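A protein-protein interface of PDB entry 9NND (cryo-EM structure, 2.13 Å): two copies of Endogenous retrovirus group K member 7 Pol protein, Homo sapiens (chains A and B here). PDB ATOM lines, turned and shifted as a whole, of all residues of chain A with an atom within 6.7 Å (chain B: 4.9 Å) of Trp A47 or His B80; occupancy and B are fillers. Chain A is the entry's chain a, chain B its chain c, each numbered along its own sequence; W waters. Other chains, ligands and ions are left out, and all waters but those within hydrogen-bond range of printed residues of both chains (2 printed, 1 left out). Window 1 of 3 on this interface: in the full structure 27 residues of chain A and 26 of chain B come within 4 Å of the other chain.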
ATOM      1  N   PHE A   3       3.739  -3.563  10.607  1.00  0.00           N
ATOM      2  CA  PHE A   3       2.587  -2.682  10.717  1.00  0.00           C
ATOM      3  C   PHE A   3       1.342  -3.490  11.047  1.00  0.00           C
ATOM      4  O   PHE A   3       1.223  -4.661  10.679  1.00  0.00           O
ATOM      5  CB  PHE A   3       2.350  -1.884   9.425  1.00  0.00           C
ATOM      6  CG  PHE A   3       3.553  -1.124   8.944  1.00  0.00           C
ATOM      7  CD1 PHE A   3       3.762   0.186   9.335  1.00  0.00           C
ATOM      8  CD2 PHE A   3       4.466  -1.715   8.087  1.00  0.00           C
ATOM      9  CE1 PHE A   3       4.864   0.889   8.893  1.00  0.00           C
ATOM     10  CE2 PHE A   3       5.569  -1.016   7.641  1.00  0.00           C
ATOM     11  CZ  PHE A   3       5.767   0.288   8.042  1.00  0.00           C
ATOM     12  N   LEU A   5      -2.291  -3.127  10.013  1.00  0.00           N
ATOM     13  CA  LEU A   5      -3.133  -2.419   9.049  1.00  0.00           C
ATOM     14  C   LEU A   5      -4.601  -2.550   9.458  1.00  0.00           C
ATOM     15  O   LEU A   5      -5.415  -3.202   8.804  1.00  0.00           O
ATOM     16  CB  LEU A   5      -2.886  -2.949   7.642  1.00  0.00           C
ATOM     17  CG  LEU A   5      -1.428  -3.026   7.185  1.00  0.00           C
ATOM     18  CD1 LEU A   5      -1.273  -4.022   6.046  1.00  0.00           C
ATOM     19  CD2 LEU A   5      -0.919  -1.653   6.773  1.00  0.00           C
ATOM     20  N   LEU A  12      -3.631  -6.636   3.169  1.00  0.00           N
ATOM     21  CA  LEU A  12      -2.740  -7.237   2.182  1.00  0.00           C
ATOM     22  C   LEU A  12      -3.390  -8.439   1.507  1.00  0.00           C
ATOM     23  O   LEU A  12      -3.246  -8.634   0.291  1.00  0.00           O
ATOM     24  CB  LEU A  12      -1.422  -7.636   2.846  1.00  0.00           C
ATOM     25  CG  LEU A  12      -0.267  -8.023   1.923  1.00  0.00           C
ATOM     26  CD1 LEU A  12       0.106  -6.871   1.008  1.00  0.00           C
ATOM     27  CD2 LEU A  12       0.935  -8.483   2.737  1.00  0.00           C
ATOM     28  N   VAL A  15      -5.841  -7.258  -1.140  1.00  0.00           N
ATOM     29  CA  VAL A  15      -5.131  -6.685  -2.282  1.00  0.00           C
ATOM     30  C   VAL A  15      -4.604  -7.793  -3.188  1.00  0.00           C
ATOM     31  O   VAL A  15      -4.879  -7.814  -4.397  1.00  0.00           O
ATOM     32  CB  VAL A  15      -3.999  -5.758  -1.797  1.00  0.00           C
ATOM     33  CG1 VAL A  15      -3.001  -5.499  -2.913  1.00  0.00           C
ATOM     34  CG2 VAL A  15      -4.567  -4.448  -1.271  1.00  0.00           C
ATOM     35  N   ASN A  42      -4.662  -0.490  -5.731  1.00  0.00           N
ATOM     36  CA  ASN A  42      -4.976  -0.796  -4.339  1.00  0.00           C
ATOM     37  C   ASN A  42      -3.722  -1.157  -3.550  1.00  0.00           C
ATOM     38  O   ASN A  42      -3.587  -0.776  -2.384  1.00  0.00           O
ATOM     39  CB  ASN A  42      -6.016  -1.912  -4.266  1.00  0.00           C
ATOM     40  CG  ASN A  42      -7.382  -1.451  -4.720  1.00  0.00           C
ATOM     41  OD1 ASN A  42      -7.719  -0.274  -4.601  1.00  0.00           O
ATOM     42  ND2 ASN A  42      -8.176  -2.369  -5.243  1.00  0.00           N
ATOM     43  N   SER A  43      -2.791  -1.885  -4.169  1.00  0.00           N
ATOM     44  CA  SER A  43      -1.528  -2.178  -3.501  1.00  0.00           C
ATOM     45  C   SER A  43      -0.750  -0.899  -3.215  1.00  0.00           C
ATOM     46  O   SER A  43      -0.211  -0.721  -2.113  1.00  0.00           O
ATOM     47  CB  SER A  43      -0.698  -3.138  -4.348  1.00  0.00           C
ATOM     48  OG  SER A  43       0.397  -3.645  -3.608  1.00  0.00           O
ATOM     49  N   THR A  44      -0.698   0.013  -4.190  1.00  0.00           N
ATOM     50  CA  THR A  44      -0.004   1.279  -3.969  1.00  0.00           C
ATOM     51  C   THR A  44      -0.673   2.084  -2.859  1.00  0.00           C
ATOM     52  O   THR A  44       0.010   2.654  -1.998  1.00  0.00           O
ATOM     53  CB  THR A  44       0.051   2.083  -5.267  1.00  0.00           C
ATOM     54  OG1 THR A  44       0.524   1.238  -6.322  1.00  0.00           O
ATOM     55  CG2 THR A  44       0.994   3.271  -5.127  1.00  0.00           C
ATOM     56  N   ARG A  45      -2.007   2.112  -2.844  1.00  0.00           N
ATOM     57  CA  ARG A  45      -2.734   2.818  -1.794  1.00  0.00           C
ATOM     58  C   ARG A  45      -2.433   2.227  -0.422  1.00  0.00           C
ATOM     59  O   ARG A  45      -2.195   2.960   0.543  1.00  0.00           O
ATOM     60  CB  ARG A  45      -4.235   2.776  -2.080  1.00  0.00           C
ATOM     61  CG  ARG A  45      -5.088   3.451  -1.018  1.00  0.00           C
ATOM     62  CD  ARG A  45      -6.568   3.352  -1.347  1.00  0.00           C
ATOM     63  NE  ARG A  45      -7.029   1.971  -1.387  1.00  0.00           N
ATOM     64  CZ  ARG A  45      -8.210   1.588  -1.854  1.00  0.00           C
ATOM     65  NH1 ARG A  45      -9.081   2.461  -2.331  1.00  0.00           N
ATOM     66  NH2 ARG A  45      -8.526   0.296  -1.840  1.00  0.00           N
ATOM     67  N   LEU A  46      -2.441   0.897  -0.319  1.00  0.00           N
ATOM     68  CA  LEU A  46      -2.157   0.257   0.962  1.00  0.00           C
ATOM     69  C   LEU A  46      -0.747   0.581   1.436  1.00  0.00           C
ATOM     70  O   LEU A  46      -0.533   0.871   2.619  1.00  0.00           O
ATOM     71  CB  LEU A  46      -2.356  -1.254   0.853  1.00  0.00           C
ATOM     72  CG  LEU A  46      -1.801  -2.093   2.006  1.00  0.00           C
ATOM     73  CD1 LEU A  46      -2.463  -1.720   3.327  1.00  0.00           C
ATOM     74  CD2 LEU A  46      -1.971  -3.577   1.721  1.00  0.00           C
ATOM     75  N   TRP A  47       0.224   0.560   0.528  1.00  0.00           N
ATOM     76  CA  TRP A  47       1.597   0.836   0.931  1.00  0.00           C
ATOM     77  C   TRP A  47       1.915   2.325   0.982  1.00  0.00           C
ATOM     78  O   TRP A  47       3.061   2.688   1.260  1.00  0.00           O
ATOM     79  CB  TRP A  47       2.570   0.099   0.009  1.00  0.00           C
ATOM     80  CG  TRP A  47       2.493  -1.376   0.228  1.00  0.00           C
ATOM     81  CD1 TRP A  47       2.083  -2.319  -0.667  1.00  0.00           C
ATOM     82  CD2 TRP A  47       2.792  -2.079   1.441  1.00  0.00           C
ATOM     83  NE1 TRP A  47       2.126  -3.565  -0.094  1.00  0.00           N
ATOM     84  CE2 TRP A  47       2.559  -3.446   1.200  1.00  0.00           C
ATOM     85  CE3 TRP A  47       3.247  -1.685   2.705  1.00  0.00           C
ATOM     86  CZ2 TRP A  47       2.762  -4.420   2.174  1.00  0.00           C
ATOM     87  CZ3 TRP A  47       3.447  -2.653   3.669  1.00  0.00           C
ATOM     88  CH2 TRP A  47       3.205  -4.005   3.399  1.00  0.00           C
ATOM     89  N   ASN A  48       0.936   3.191   0.723  1.00  0.00           N
ATOM     90  CA  ASN A  48       1.076   4.616   0.981  1.00  0.00           C
ATOM     91  C   ASN A  48       0.176   5.089   2.118  1.00  0.00           C
ATOM     92  O   ASN A  48      -0.074   6.290   2.248  1.00  0.00           O
ATOM     93  CB  ASN A  48       0.794   5.413  -0.292  1.00  0.00           C
ATOM     94  CG  ASN A  48       1.995   5.484  -1.205  1.00  0.00           C
ATOM     95  OD1 ASN A  48       2.834   6.372  -1.073  1.00  0.00           O
ATOM     96  ND2 ASN A  48       2.091   4.542  -2.133  1.00  0.00           N
ATOM     97  N   SER A  49      -0.312   4.169   2.953  1.00  0.00           N
ATOM     98  CA  SER A  49      -1.312   4.506   3.955  1.00  0.00           C
ATOM     99  C   SER A  49      -0.989   4.051   5.371  1.00  0.00           C
ATOM    100  O   SER A  49      -1.733   4.412   6.287  1.00  0.00           O
ATOM    101  CB  SER A  49      -2.679   3.926   3.561  1.00  0.00           C
ATOM    102  OG  SER A  49      -2.720   2.530   3.788  1.00  0.00           O
ATOM    103  N   GLN A  50       0.066   3.271   5.586  1.00  0.00           N
ATOM    104  CA  GLN A  50       0.407   2.861   6.941  1.00  0.00           C
ATOM    105  C   GLN A  50       0.837   4.071   7.765  1.00  0.00           C
ATOM    106  O   GLN A  50       1.518   4.972   7.270  1.00  0.00           O
ATOM    107  CB  GLN A  50       1.506   1.797   6.923  1.00  0.00           C
ATOM    108  CG  GLN A  50       2.822   2.251   6.335  1.00  0.00           C
ATOM    109  CD  GLN A  50       3.026   1.770   4.916  1.00  0.00           C
ATOM    110  OE1 GLN A  50       2.261   2.112   4.019  1.00  0.00           O
ATOM    111  NE2 GLN A  50       4.069   0.975   4.706  1.00  0.00           N
ATOM    112  N   SER A  51       0.415   4.097   9.028  1.00  0.00           N
ATOM    113  CA  SER A  51       0.629   5.261   9.882  1.00  0.00           C
ATOM    114  C   SER A  51       2.014   5.262  10.523  1.00  0.00           C
ATOM    115  O   SER A  51       2.769   6.226  10.368  1.00  0.00           O
ATOM    116  CB  SER A  51      -0.455   5.324  10.962  1.00  0.00           C
ATOM    117  OG  SER A  51      -0.354   6.522  11.711  1.00  0.00           O
ATOM    118  N   TRP A  70      15.464  -6.569   4.469  1.00  0.00           N
ATOM    119  CA  TRP A  70      14.276  -6.000   3.841  1.00  0.00           C
ATOM    120  C   TRP A  70      14.372  -4.480   3.759  1.00  0.00           C
ATOM    121  O   TRP A  70      14.038  -3.879   2.731  1.00  0.00           O
ATOM    122  CB  TRP A  70      13.032  -6.434   4.616  1.00  0.00           C
ATOM    123  CG  TRP A  70      11.746  -5.907   4.073  1.00  0.00           C
ATOM    124  CD1 TRP A  70      10.919  -6.525   3.181  1.00  0.00           C
ATOM    125  CD2 TRP A  70      11.124  -4.660   4.398  1.00  0.00           C
ATOM    126  NE1 TRP A  70       9.827  -5.736   2.924  1.00  0.00           N
ATOM    127  CE2 TRP A  70       9.928  -4.584   3.659  1.00  0.00           C
ATOM    128  CE3 TRP A  70      11.466  -3.597   5.238  1.00  0.00           C
ATOM    129  CZ2 TRP A  70       9.071  -3.489   3.734  1.00  0.00           C
ATOM    130  CZ3 TRP A  70      10.615  -2.509   5.311  1.00  0.00           C
ATOM    131  CH2 TRP A  70       9.431  -2.464   4.565  1.00  0.00           C
ATOM    132  N   ARG A  74      14.429  -2.063   0.455  1.00  0.00           N
ATOM    133  CA  ARG A  74      13.537  -0.914   0.321  1.00  0.00           C
ATOM    134  C   ARG A  74      14.316   0.372   0.066  1.00  0.00           C
ATOM    135  O   ARG A  74      13.916   1.194  -0.764  1.00  0.00           O
ATOM    136  CB  ARG A  74      12.670  -0.770   1.573  1.00  0.00           C
ATOM    137  CG  ARG A  74      11.674  -1.898   1.779  1.00  0.00           C
ATOM    138  CD  ARG A  74      10.550  -1.834   0.762  1.00  0.00           C
ATOM    139  NE  ARG A  74       9.471  -0.960   1.205  1.00  0.00           N
ATOM    140  CZ  ARG A  74       8.182  -1.263   1.134  1.00  0.00           C
ATOM    141  NH1 ARG A  74       7.769  -2.415   0.633  1.00  0.00           N
ATOM    142  NH2 ARG A  74       7.286  -0.386   1.576  1.00  0.00           N
ATOM    143  N   LEU A  78      14.150   2.731  -3.208  1.00  0.00           N
ATOM    144  CA  LEU A  78      13.846   4.157  -3.124  1.00  0.00           C
ATOM    145  C   LEU A  78      14.940   4.995  -3.777  1.00  0.00           C
ATOM    146  O   LEU A  78      14.649   5.970  -4.480  1.00  0.00           O
ATOM    147  CB  LEU A  78      13.651   4.567  -1.664  1.00  0.00           C
ATOM    148  CG  LEU A  78      13.059   5.957  -1.418  1.00  0.00           C
ATOM    149  CD1 LEU A  78      11.806   6.169  -2.246  1.00  0.00           C
ATOM    150  CD2 LEU A  78      12.772   6.164   0.061  1.00  0.00           C
ATOM    151  N   MET B  76       9.956   4.666   5.955  1.00  0.00           N
ATOM    152  CA  MET B  76       8.542   4.678   5.594  1.00  0.00           C
ATOM    153  C   MET B  76       8.065   6.093   5.294  1.00  0.00           C
ATOM    154  O   MET B  76       7.342   6.324   4.315  1.00  0.00           O
ATOM    155  CB  MET B  76       7.713   4.061   6.721  1.00  0.00           C
ATOM    156  CG  MET B  76       6.221   4.007   6.443  1.00  0.00           C
ATOM    157  SD  MET B  76       5.236   4.233   7.937  1.00  0.00           S
ATOM    158  CE  MET B  76       4.838   5.974   7.814  1.00  0.00           C
ATOM    159  N   SER B  77       8.474   7.056   6.124  1.00  0.00           N
ATOM    160  CA  SER B  77       8.099   8.446   5.893  1.00  0.00           C
ATOM    161  C   SER B  77       8.673   8.964   4.580  1.00  0.00           C
ATOM    162  O   SER B  77       7.995   9.686   3.846  1.00  0.00           O
ATOM    163  CB  SER B  77       8.564   9.316   7.058  1.00  0.00           C
ATOM    164  OG  SER B  77       8.337  10.684   6.781  1.00  0.00           O
ATOM    165  N   LEU B  78       9.925   8.616   4.276  1.00  0.00           N
ATOM    166  CA  LEU B  78      10.529   9.048   3.018  1.00  0.00           C
ATOM    167  C   LEU B  78       9.815   8.431   1.822  1.00  0.00           C
ATOM    168  O   LEU B  78       9.573   9.107   0.816  1.00  0.00           O
ATOM    169  CB  LEU B  78      12.016   8.698   3.001  1.00  0.00           C
ATOM    170  CG  LEU B  78      12.863   9.340   1.898  1.00  0.00           C
ATOM    171  CD1 LEU B  78      12.613  10.835   1.813  1.00  0.00           C
ATOM    172  CD2 LEU B  78      14.339   9.054   2.123  1.00  0.00           C
ATOM    173  N   GLU B  79       9.464   7.145   1.919  1.00  0.00           N
ATOM    174  CA  GLU B  79       8.709   6.492   0.854  1.00  0.00           C
ATOM    175  C   GLU B  79       7.376   7.192   0.623  1.00  0.00           C
ATOM    176  O   GLU B  79       6.993   7.462  -0.520  1.00  0.00           O
ATOM    177  CB  GLU B  79       8.485   5.019   1.197  1.00  0.00           C
ATOM    178  CG  GLU B  79       9.715   4.146   1.055  1.00  0.00           C
ATOM    179  CD  GLU B  79       9.499   2.747   1.592  1.00  0.00           C
ATOM    180  OE1 GLU B  79       8.670   2.580   2.510  1.00  0.00           O
ATOM    181  OE2 GLU B  79      10.163   1.812   1.097  1.00  0.00           O
ATOM    182  N   HIS B  80       6.660   7.505   1.706  1.00  0.00           N
ATOM    183  CA  HIS B  80       5.379   8.190   1.561  1.00  0.00           C
ATOM    184  C   HIS B  80       5.557   9.596   0.997  1.00  0.00           C
ATOM    185  O   HIS B  80       4.761  10.041   0.163  1.00  0.00           O
ATOM    186  CB  HIS B  80       4.649   8.230   2.902  1.00  0.00           C
ATOM    187  CG  HIS B  80       4.101   6.903   3.330  1.00  0.00           C
ATOM    188  ND1 HIS B  80       3.398   6.731   4.501  1.00  0.00           N
ATOM    189  CD2 HIS B  80       4.154   5.685   2.741  1.00  0.00           C
ATOM    190  CE1 HIS B  80       3.042   5.464   4.617  1.00  0.00           C
ATOM    191  NE2 HIS B  80       3.489   4.807   3.562  1.00  0.00           N
ATOM    192  N   ARG B  81       6.600  10.306   1.435  1.00  0.00           N
ATOM    193  CA  ARG B  81       6.840  11.661   0.951  1.00  0.00           C
ATOM    194  C   ARG B  81       7.162  11.668  -0.535  1.00  0.00           C
ATOM    195  O   ARG B  81       6.752  12.580  -1.261  1.00  0.00           O
ATOM    196  CB  ARG B  81       7.977  12.307   1.743  1.00  0.00           C
ATOM    197  CG  ARG B  81       7.587  12.769   3.133  1.00  0.00           C
ATOM    198  CD  ARG B  81       8.808  13.179   3.934  1.00  0.00           C
ATOM    199  NE  ARG B  81       9.521  14.278   3.298  1.00  0.00           N
ATOM    200  CZ  ARG B  81      10.800  14.561   3.498  1.00  0.00           C
ATOM    201  NH1 ARG B  81      11.545  13.842   4.321  1.00  0.00           N
ATOM    202  NH2 ARG B  81      11.342  15.595   2.864  1.00  0.00           N
ATOM    203  N   PHE B  82       7.896  10.658  -1.007  1.00  0.00           N
ATOM    204  CA  PHE B  82       8.273  10.617  -2.416  1.00  0.00           C
ATOM    205  C   PHE B  82       7.055  10.601  -3.332  1.00  0.00           C
ATOM    206  O   PHE B  82       7.131  11.080  -4.468  1.00  0.00           O
ATOM    207  CB  PHE B  82       9.156   9.404  -2.696  1.00  0.00           C
ATOM    208  CG  PHE B  82       9.608   9.310  -4.123  1.00  0.00           C
ATOM    209  CD1 PHE B  82      10.370  10.318  -4.686  1.00  0.00           C
ATOM    210  CD2 PHE B  82       9.253   8.226  -4.907  1.00  0.00           C
ATOM    211  CE1 PHE B  82      10.781  10.243  -6.003  1.00  0.00           C
ATOM    212  CE2 PHE B  82       9.661   8.145  -6.225  1.00  0.00           C
ATOM    213  CZ  PHE B  82      10.426   9.156  -6.773  1.00  0.00           C
ATOM    214  N   GLN B  83       5.931  10.065  -2.868  1.00  0.00           N
ATOM    215  CA  GLN B  83       4.733   9.959  -3.689  1.00  0.00           C
ATOM    216  C   GLN B  83       3.709  11.053  -3.410  1.00  0.00           C
ATOM    217  O   GLN B  83       2.669  11.084  -4.072  1.00  0.00           O
ATOM    218  CB  GLN B  83       4.092   8.579  -3.505  1.00  0.00           C
ATOM    219  CG  GLN B  83       4.838   7.476  -4.242  1.00  0.00           C
ATOM    220  CD  GLN B  83       3.961   6.291  -4.587  1.00  0.00           C
ATOM    221  OE1 GLN B  83       4.126   5.203  -4.039  1.00  0.00           O
ATOM    222  NE2 GLN B  83       3.028   6.494  -5.508  1.00  0.00           N
ATOM    223  N   LEU B  84       3.977  11.950  -2.464  1.00  0.00           N
ATOM    224  CA  LEU B  84       3.045  13.030  -2.167  1.00  0.00           C
ATOM    225  C   LEU B  84       3.068  14.092  -3.264  1.00  0.00           C
ATOM    226  O   LEU B  84       4.095  14.342  -3.898  1.00  0.00           O
ATOM    227  CB  LEU B  84       3.383  13.678  -0.823  1.00  0.00           C
ATOM    228  CG  LEU B  84       3.011  12.935   0.462  1.00  0.00           C
ATOM    229  CD1 LEU B  84       3.341  13.788   1.681  1.00  0.00           C
ATOM    230  CD2 LEU B  84       1.544  12.533   0.459  1.00  0.00           C
ATOM    231  N   LYS B 129      -4.427   9.483   4.956  1.00  0.00           N
ATOM    232  CA  LYS B 129      -3.472   9.172   3.898  1.00  0.00           C
ATOM    233  C   LYS B 129      -4.158   8.488   2.725  1.00  0.00           C
ATOM    234  O   LYS B 129      -3.821   8.748   1.566  1.00  0.00           O
ATOM    235  CB  LYS B 129      -2.337   8.308   4.445  1.00  0.00           C
ATOM    236  CG  LYS B 129      -1.276   9.096   5.186  1.00  0.00           C
ATOM    237  CD  LYS B 129      -0.160   8.197   5.689  1.00  0.00           C
ATOM    238  CE  LYS B 129       1.043   9.014   6.123  1.00  0.00           C
ATOM    239  NZ  LYS B 129       2.114   8.171   6.719  1.00  0.00           N
HETATM  240  O   HOH W   1       2.259   9.043  -0.225  1.00  0.00           O
HETATM  241  O   HOH W   2       5.486   2.054   2.432  1.00  0.00           O
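The side-chain amide nitrogen (ND2) of Asn A48 sits at hydrogen-bond distance from the side-chain amide oxygen (OE1) of Gln B83, 2.9 Å away. The backbone carbonyl oxygen (O) of Trp A47 lies within hydrogen-bond range of a ring nitrogen (NE2) of His B80 (3.2 Å). The side-chain amide oxygen (OE1) of Gln A50 sits at hydrogen-bond distance from a ring nitrogen (NE2) of His B80 (3.0 Å). O of Gln A50 is in hydrogen-bond range of NZ of Lys B129. OE2 of Glu B79 lies within salt-bridge range of NE of Arg A74 (2.9 Å).
The backbone carbonyl oxygen (O) of Thr A44 sits at hydrogen-bond distance from the side-chain amide nitrogen (ND2) of Asn A48 (2.8 Å). The backbone carbonyl oxygen (O) of Trp A47 sits close to the side-chain amide oxygen (OE1) of Gln A50 (2.9 Å). The backbone carbonyl oxygen of Leu A46 lies within hydrogen-bond range of the side-chain hydroxyl of Ser A49 (3.0 Å). O of Leu A46 sits close to OE1 of Gln A50, 3.4 Å away. The backbone carbonyl oxygen of Arg A45 lies close to the side-chain hydroxyl of Ser A49 (3.3 Å). A ring nitrogen (ND1) of His B80 sits at hydrogen-bond distance from the side-chain amino group (NZ) of Lys B129, at 2.9 Å.
Phe A3 touches Met B76. NE2 of Gln B83 touches CG2 of Thr A44, 3.8 Å away. His B80 touches Asn A48. Lys B129 touches Asn A48. NE2 of His B80 touches N of Ser A49 (3.9 Å). Ser A49 touches Lys B129 (CA to CB, 3.97 Å). SD of Met B76 touches CG of Gln A50, at 3.5 Å. O of Ser A51 touches CE of Met B76, 3.3 Å away. CD2 of Leu A78 touches CG of Leu B78, 3.7 Å away. Leu A78 touches Glu B79.
Of the printed residues of chain B, Trp A47 touches His B80 (3.2 Å). His B80 touches just these residues of chain A: Trp A47 (3.2 Å), Asn A48 (3.5 Å), Ser A49 (3.9 Å) and Gln A50 (3.0 Å). Of the printed residues of chain B, Ser A49 touches His B80 (3.9 Å) and Lys B129 (3.97 Å). Of the printed residues of chain B, Gln A50 touches Met B76 (3.5 Å), His B80 (3.0 Å) and Lys B129 (3.3 Å). Ser B77 touches none of the printed residues of chain A. Arg A45 touches none of the printed residues of chain B. The nearest printed residue of chain B that does not touch Trp A47 is Glu B79 (5.7 Å). The nearest residue of chain A that does not touch His B80 is Ser A51 (5.3 Å).
Hydrophobic or aromatic side chains of chain A that line the printed part of chain B: Phe A3 and Leu A78. Of the 10 printed residues of chain B, 6 touch a printed residue of chain A. Printed residues of chain B that touch a printed residue of chain A: Met B76, Leu B78, Glu B79, His B80, Gln B83 and Lys B129. Hydrophobic or aromatic side chains of chain B within 4 Å of the printed part of chain A: Met B76, Leu B78 and His B80. Among the printed residues, 15 pairs touch across the chains. Among the printed residues, Asp or Glu carboxylates within 4 Å of a Lys or Arg side-chain nitrogen of the other chain: Arg A74 with Glu B79 (2.9 Å).
Leu B78 touches its own counterpart, Leu A78. Of the 15 pairs that touch across the chains among the printed residues, 1 has its exchanged pair printed and touching as well.
Water W1 bridges O of His B80 (2.7 Å) and OD1 of Asn A48 (2.9 Å). Water W2 lies within hydrogen-bond range of the backbone carbonyl oxygen (O) of Trp A47 (2.8 Å), the side-chain amide nitrogen (NE2) of Gln A50 (2.9 Å), the guanidinium group (NH2) of Arg A74 (3.2 Å) and the side-chain carboxylate (OE1) of Glu B79 (3.2 Å).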
